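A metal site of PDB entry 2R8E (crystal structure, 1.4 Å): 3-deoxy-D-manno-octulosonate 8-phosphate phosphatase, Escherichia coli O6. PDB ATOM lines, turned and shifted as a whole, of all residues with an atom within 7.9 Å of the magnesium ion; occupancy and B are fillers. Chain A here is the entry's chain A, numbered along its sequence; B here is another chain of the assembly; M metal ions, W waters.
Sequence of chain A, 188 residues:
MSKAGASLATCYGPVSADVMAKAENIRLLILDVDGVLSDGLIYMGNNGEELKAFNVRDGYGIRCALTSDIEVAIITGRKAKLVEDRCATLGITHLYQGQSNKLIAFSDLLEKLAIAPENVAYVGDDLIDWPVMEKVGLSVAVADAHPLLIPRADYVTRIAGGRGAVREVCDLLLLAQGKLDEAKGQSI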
ATOM      1  N   LEU A  31       7.205 -12.900 -33.332  1.00  0.00           N
ATOM      2  CA  LEU A  31       6.397 -12.639 -32.142  1.00  0.00           C
ATOM      3  C   LEU A  31       4.954 -12.427 -32.489  1.00  0.00           C
ATOM      4  O   LEU A  31       4.616 -11.578 -33.320  1.00  0.00           O
ATOM      5  CB  LEU A  31       6.906 -11.378 -31.446  1.00  0.00           C
ATOM      6  CG  LEU A  31       8.366 -11.392 -31.012  1.00  0.00           C
ATOM      7  CD1 LEU A  31       8.800 -10.037 -30.496  1.00  0.00           C
ATOM      8  CD2 LEU A  31       8.584 -12.474 -29.953  1.00  0.00           C
ATOM      9  N   ASP A  32       4.089 -13.195 -31.864  1.00  0.00           N
ATOM     10  CA  ASP A  32       2.663 -12.926 -31.926  1.00  0.00           C
ATOM     11  C   ASP A  32       2.388 -11.647 -31.135  1.00  0.00           C
ATOM     12  O   ASP A  32       3.110 -11.342 -30.169  1.00  0.00           O
ATOM     13  CB  ASP A  32       1.916 -14.104 -31.321  1.00  0.00           C
ATOM     14  CG  ASP A  32       0.427 -13.917 -31.332  1.00  0.00           C
ATOM     15  OD1 ASP A  32      -0.192 -14.163 -30.253  1.00  0.00           O
ATOM     16  OD2 ASP A  32      -0.121 -13.557 -32.398  1.00  0.00           O
ATOM     17  N   VAL A  33       1.364 -10.899 -31.521  1.00  0.00           N
ATOM     18  CA  VAL A  33       1.026  -9.709 -30.765  1.00  0.00           C
ATOM     19  C   VAL A  33       0.101 -10.010 -29.563  1.00  0.00           C
ATOM     20  O   VAL A  33       0.526  -9.867 -28.396  1.00  0.00           O
ATOM     21  CB  VAL A  33       0.409  -8.612 -31.647  1.00  0.00           C
ATOM     22  CG1 VAL A  33      -0.077  -7.416 -30.799  1.00  0.00           C
ATOM     23  CG2 VAL A  33       1.427  -8.166 -32.725  1.00  0.00           C
ATOM     24  N   ASP A  34      -1.151 -10.380 -29.826  1.00  0.00           N
ATOM     25  CA  ASP A  34      -2.141 -10.461 -28.754  1.00  0.00           C
ATOM     26  C   ASP A  34      -1.850 -11.628 -27.822  1.00  0.00           C
ATOM     27  O   ASP A  34      -1.795 -12.786 -28.263  1.00  0.00           O
ATOM     28  CB  ASP A  34      -3.532 -10.568 -29.324  1.00  0.00           C
ATOM     29  CG  ASP A  34      -3.867  -9.403 -30.226  1.00  0.00           C
ATOM     30  OD1 ASP A  34      -3.915  -8.267 -29.749  1.00  0.00           O
ATOM     31  OD2 ASP A  34      -4.056  -9.630 -31.433  1.00  0.00           O
ATOM     32  N   GLY A  35      -1.654 -11.318 -26.534  1.00  0.00           N
ATOM     33  CA  GLY A  35      -1.411 -12.335 -25.502  1.00  0.00           C
ATOM     34  C   GLY A  35       0.050 -12.727 -25.392  1.00  0.00           C
ATOM     35  O   GLY A  35       0.400 -13.565 -24.568  1.00  0.00           O
ATOM     36  N   VAL A  36       0.903 -12.130 -26.232  1.00  0.00           N
ATOM     37  CA  VAL A  36       2.348 -12.392 -26.199  1.00  0.00           C
ATOM     38  C   VAL A  36       3.058 -11.061 -25.923  1.00  0.00           C
ATOM     39  O   VAL A  36       3.624 -10.848 -24.819  1.00  0.00           O
ATOM     40  CB  VAL A  36       2.830 -13.089 -27.490  1.00  0.00           C
ATOM     41  CG1 VAL A  36       4.351 -13.134 -27.546  1.00  0.00           C
ATOM     42  CG2 VAL A  36       2.254 -14.490 -27.547  1.00  0.00           C
ATOM     43  N   LEU A  37       2.991 -10.142 -26.879  1.00  0.00           N
ATOM     44  CA  LEU A  37       3.449  -8.782 -26.669  1.00  0.00           C
ATOM     45  C   LEU A  37       2.493  -7.972 -25.792  1.00  0.00           C
ATOM     46  O   LEU A  37       2.887  -7.008 -25.170  1.00  0.00           O
ATOM     47  CB  LEU A  37       3.636  -8.074 -28.015  1.00  0.00           C
ATOM     48  CG  LEU A  37       4.908  -8.515 -28.741  1.00  0.00           C
ATOM     49  CD1 LEU A  37       4.839  -8.124 -30.213  1.00  0.00           C
ATOM     50  CD2 LEU A  37       6.149  -7.883 -28.066  1.00  0.00           C
ATOM     51  N   SER A  38       1.223  -8.362 -25.754  1.00  0.00           N
ATOM     52  CA  SER A  38       0.202  -7.667 -24.991  1.00  0.00           C
ATOM     53  C   SER A  38      -0.325  -8.563 -23.906  1.00  0.00           C
ATOM     54  O   SER A  38      -0.072  -9.770 -23.886  1.00  0.00           O
ATOM     55  CB  SER A  38      -0.973  -7.263 -25.876  1.00  0.00           C
ATOM     56  OG  SER A  38      -1.814  -8.389 -26.085  1.00  0.00           O
ATOM     57  N   GLY A  40      -3.235  -9.541 -23.788  1.00  0.00           N
ATOM     58  CA  GLY A  40      -4.356 -10.306 -24.345  1.00  0.00           C
ATOM     59  C   GLY A  40      -5.638  -9.516 -24.509  1.00  0.00           C
ATOM     60  O   GLY A  40      -6.646 -10.054 -24.963  1.00  0.00           O
ATOM     61  N   LYS A 102      -0.723 -17.892 -40.789  1.00  0.00           N
ATOM     62  CA  LYS A 102       0.575 -17.399 -40.476  1.00  0.00           C
ATOM     63  C   LYS A 102       1.626 -18.029 -41.364  1.00  0.00           C
ATOM     64  O   LYS A 102       2.704 -17.462 -41.553  1.00  0.00           O
ATOM     65  CB  LYS A 102       0.839 -17.495 -38.994  1.00  0.00           C
ATOM     66  CG  LYS A 102      -0.244 -16.736 -38.276  1.00  0.00           C
ATOM     67  CD  LYS A 102       0.256 -16.131 -37.017  1.00  0.00           C
ATOM     68  CE  LYS A 102      -0.892 -15.530 -36.289  1.00  0.00           C
ATOM     69  NZ  LYS A 102      -0.972 -14.068 -36.562  1.00  0.00           N
ATOM     70  N   TYR A 122       9.577 -18.815 -32.497  1.00  0.00           N
ATOM     71  CA  TYR A 122       8.237 -18.202 -32.563  1.00  0.00           C
ATOM     72  C   TYR A 122       7.631 -18.250 -31.190  1.00  0.00           C
ATOM     73  O   TYR A 122       7.650 -19.303 -30.568  1.00  0.00           O
ATOM     74  CB  TYR A 122       7.333 -18.972 -33.523  1.00  0.00           C
ATOM     75  CG  TYR A 122       5.976 -18.337 -33.764  1.00  0.00           C
ATOM     76  CD1 TYR A 122       5.678 -17.728 -34.990  1.00  0.00           C
ATOM     77  CD2 TYR A 122       4.974 -18.333 -32.778  1.00  0.00           C
ATOM     78  CE1 TYR A 122       4.462 -17.172 -35.249  1.00  0.00           C
ATOM     79  CE2 TYR A 122       3.745 -17.759 -33.027  1.00  0.00           C
ATOM     80  CZ  TYR A 122       3.488 -17.190 -34.267  1.00  0.00           C
ATOM     81  OH  TYR A 122       2.275 -16.622 -34.544  1.00  0.00           O
ATOM     82  N   VAL A 123       7.072 -17.126 -30.737  1.00  0.00           N
ATOM     83  CA  VAL A 123       6.433 -17.060 -29.424  1.00  0.00           C
ATOM     84  C   VAL A 123       4.930 -16.810 -29.624  1.00  0.00           C
ATOM     85  O   VAL A 123       4.553 -15.789 -30.205  1.00  0.00           O
ATOM     86  CB  VAL A 123       7.020 -15.911 -28.570  1.00  0.00           C
ATOM     87  CG1 VAL A 123       6.485 -15.995 -27.138  1.00  0.00           C
ATOM     88  CG2 VAL A 123       8.571 -15.981 -28.555  1.00  0.00           C
ATOM     89  N   GLY A 124       4.098 -17.756 -29.144  1.00  0.00           N
ATOM     90  CA  GLY A 124       2.642 -17.689 -29.309  1.00  0.00           C
ATOM     91  C   GLY A 124       1.870 -17.907 -28.030  1.00  0.00           C
ATOM     92  O   GLY A 124       2.449 -18.277 -27.004  1.00  0.00           O
ATOM     93  N   ASP A 125       0.553 -17.658 -28.108  1.00  0.00           N
ATOM     94  CA  ASP A 125      -0.333 -17.892 -26.967  1.00  0.00           C
ATOM     95  C   ASP A 125      -1.589 -18.661 -27.321  1.00  0.00           C
ATOM     96  O   ASP A 125      -2.351 -18.954 -26.408  1.00  0.00           O
ATOM     97  CB  ASP A 125      -0.735 -16.587 -26.259  1.00  0.00           C
ATOM     98  CG  ASP A 125      -1.781 -15.805 -27.012  1.00  0.00           C
ATOM     99  OD1 ASP A 125      -2.778 -15.352 -26.402  1.00  0.00           O
ATOM    100  OD2 ASP A 125      -1.586 -15.654 -28.242  1.00  0.00           O
ATOM    101  N   ASP A 126      -1.834 -19.002 -28.596  1.00  0.00           N
ATOM    102  CA  ASP A 126      -3.116 -19.653 -28.929  1.00  0.00           C
ATOM    103  C   ASP A 126      -2.906 -20.694 -30.019  1.00  0.00           C
ATOM    104  O   ASP A 126      -1.835 -20.792 -30.599  1.00  0.00           O
ATOM    105  CB  ASP A 126      -4.186 -18.618 -29.339  1.00  0.00           C
ATOM    106  CG  ASP A 126      -5.613 -19.063 -29.037  1.00  0.00           C
ATOM    107  OD1 ASP A 126      -5.825 -20.250 -28.667  1.00  0.00           O
ATOM    108  OD2 ASP A 126      -6.541 -18.253 -29.225  1.00  0.00           O
ATOM    109  N   LEU A 127      -3.956 -21.457 -30.280  1.00  0.00           N
ATOM    110  CA  LEU A 127      -3.870 -22.575 -31.226  1.00  0.00           C
ATOM    111  C   LEU A 127      -3.539 -22.111 -32.644  1.00  0.00           C
ATOM    112  O   LEU A 127      -2.921 -22.868 -33.415  1.00  0.00           O
ATOM    113  CB  LEU A 127      -5.190 -23.355 -31.204  1.00  0.00           C
ATOM    114  CG  LEU A 127      -5.406 -24.041 -29.853  1.00  0.00           C
ATOM    115  CD1 LEU A 127      -6.738 -24.804 -29.820  1.00  0.00           C
ATOM    116  CD2 LEU A 127      -4.230 -24.960 -29.502  1.00  0.00           C
ATOM    117  N   ILE A 128      -3.972 -20.908 -32.988  1.00  0.00           N
ATOM    118  CA  ILE A 128      -3.667 -20.353 -34.318  1.00  0.00           C
ATOM    119  C   ILE A 128      -2.174 -20.183 -34.556  1.00  0.00           C
ATOM    120  O   ILE A 128      -1.720 -20.083 -35.700  1.00  0.00           O
ATOM    121  CB  ILE A 128      -4.432 -19.043 -34.606  1.00  0.00           C
ATOM    122  CG1 ILE A 128      -4.110 -17.982 -33.539  1.00  0.00           C
ATOM    123  CG2 ILE A 128      -5.922 -19.345 -34.736  1.00  0.00           C
ATOM    124  CD1 ILE A 128      -4.777 -16.629 -33.795  1.00  0.00           C
ATOM    125  N   ASP A 129      -1.386 -20.179 -33.478  1.00  0.00           N
ATOM    126  CA  ASP A 129       0.063 -20.028 -33.593  1.00  0.00           C
ATOM    127  C   ASP A 129       0.766 -21.357 -33.847  1.00  0.00           C
ATOM    128  O   ASP A 129       1.939 -21.386 -34.207  1.00  0.00           O
ATOM    129  CB  ASP A 129       0.609 -19.453 -32.292  1.00  0.00           C
ATOM    130  CG  ASP A 129       0.103 -18.042 -32.042  1.00  0.00           C
ATOM    131  OD1 ASP A 129       0.271 -17.192 -32.940  1.00  0.00           O
ATOM    132  OD2 ASP A 129      -0.481 -17.821 -30.947  1.00  0.00           O
ATOM    133  N   VAL A 142       3.806 -18.746 -24.124  1.00  0.00           N
ATOM    134  CA  VAL A 142       3.882 -17.923 -22.915  1.00  0.00           C
ATOM    135  C   VAL A 142       3.219 -18.625 -21.727  1.00  0.00           C
ATOM    136  O   VAL A 142       2.393 -19.548 -21.907  1.00  0.00           O
ATOM    137  CB  VAL A 142       3.326 -16.493 -23.152  1.00  0.00           C
ATOM    138  CG1 VAL A 142       4.106 -15.838 -24.279  1.00  0.00           C
ATOM    139  CG2 VAL A 142       1.844 -16.524 -23.455  1.00  0.00           C
ATOM    140  N   LEU A 149      -2.057 -25.212 -25.985  1.00  0.00           N
ATOM    141  CA  LEU A 149      -0.805 -24.892 -26.644  1.00  0.00           C
ATOM    142  C   LEU A 149       0.393 -25.252 -25.779  1.00  0.00           C
ATOM    143  O   LEU A 149       1.448 -25.670 -26.287  1.00  0.00           O
ATOM    144  CB  LEU A 149      -0.741 -23.398 -26.994  1.00  0.00           C
ATOM    145  CG  LEU A 149       0.468 -22.992 -27.837  1.00  0.00           C
ATOM    146  CD1 LEU A 149       0.347 -23.592 -29.275  1.00  0.00           C
ATOM    147  CD2 LEU A 149       0.602 -21.465 -27.871  1.00  0.00           C
ATOM    148  N   VAL B  56      -8.872 -11.142 -26.434  1.00  0.00           N
ATOM    149  CA  VAL B  56      -8.680 -11.626 -27.796  1.00  0.00           C
ATOM    150  C   VAL B  56      -8.902 -13.133 -27.915  1.00  0.00           C
ATOM    151  O   VAL B  56      -9.525 -13.602 -28.888  1.00  0.00           O
ATOM    152  CB  VAL B  56      -7.307 -11.184 -28.353  1.00  0.00           C
ATOM    153  CG1 VAL B  56      -6.997 -11.820 -29.700  1.00  0.00           C
ATOM    154  CG2 VAL B  56      -7.272  -9.653 -28.473  1.00  0.00           C
ATOM    155  N   ARG B  57      -8.415 -13.930 -26.949  1.00  0.00           N
ATOM    156  CA  ARG B  57      -8.650 -15.368 -27.060  1.00  0.00           C
ATOM    157  C   ARG B  57     -10.159 -15.714 -26.915  1.00  0.00           C
ATOM    158  O   ARG B  57     -10.631 -16.715 -27.507  1.00  0.00           O
ATOM    159  CB  ARG B  57      -7.783 -16.178 -26.086  1.00  0.00           C
ATOM    160  CG  ARG B  57      -6.303 -16.120 -26.404  1.00  0.00           C
ATOM    161  CD  ARG B  57      -5.531 -17.373 -25.986  1.00  0.00           C
ATOM    162  NE  ARG B  57      -5.615 -17.693 -24.566  1.00  0.00           N
ATOM    163  CZ  ARG B  57      -4.703 -17.336 -23.654  1.00  0.00           C
ATOM    164  NH1 ARG B  57      -4.885 -17.686 -22.395  1.00  0.00           N
ATOM    165  NH2 ARG B  57      -3.596 -16.676 -24.000  1.00  0.00           N
HETATM  166 MG    MG M   1      -2.128 -14.309 -29.654  1.00  0.00          MG
HETATM  167  O   HOH W   1      -2.409 -15.907 -30.976  1.00  0.00           O
HETATM  168  O   HOH W   2      -2.472 -12.951 -31.344  1.00  0.00           O
HETATM  169  O   HOH W   3      -4.081 -14.201 -29.256  1.00  0.00           O
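Of the 22 residues printed, 3 come within 4 Å of the magnesium ion. The nearest printed residue that does not touch the magnesium ion is Asp 129 (4.1 Å).
The backbone NH of Asp 125 sits at hydrogen-bond distance from the side-chain carboxylate of Asp 129 (3.0 Å). The side-chain carboxylate (OD1) of Asp 125 lies within salt-bridge range of the guanidinium group (NH2) of Arg 57 of chain B, 2.9 Å away. N of Asp 32 lies within hydrogen-bond range of O of Val 123, 3.1 Å away.
Water W2 lies within hydrogen-bond range of OD2 of Asp 32 (2.6 Å) and N of Asp 34 (3.3 Å).
Water W3 binds the magnesium ion (2.0 Å). The side-chain carboxylate (OD2) of Asp 125 is bound to the magnesium ion (2.0 Å). OD1 of Asp 32 binds the magnesium ion, 2.0 Å away. The backbone carbonyl oxygen (O) of Asp 34 binds the magnesium ion (2.1 Å). Water W1 binds the magnesium ion. The magnesium ion is bound by water W2 (2.2 Å). The magnesium ion has six donor atoms within binding distance.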
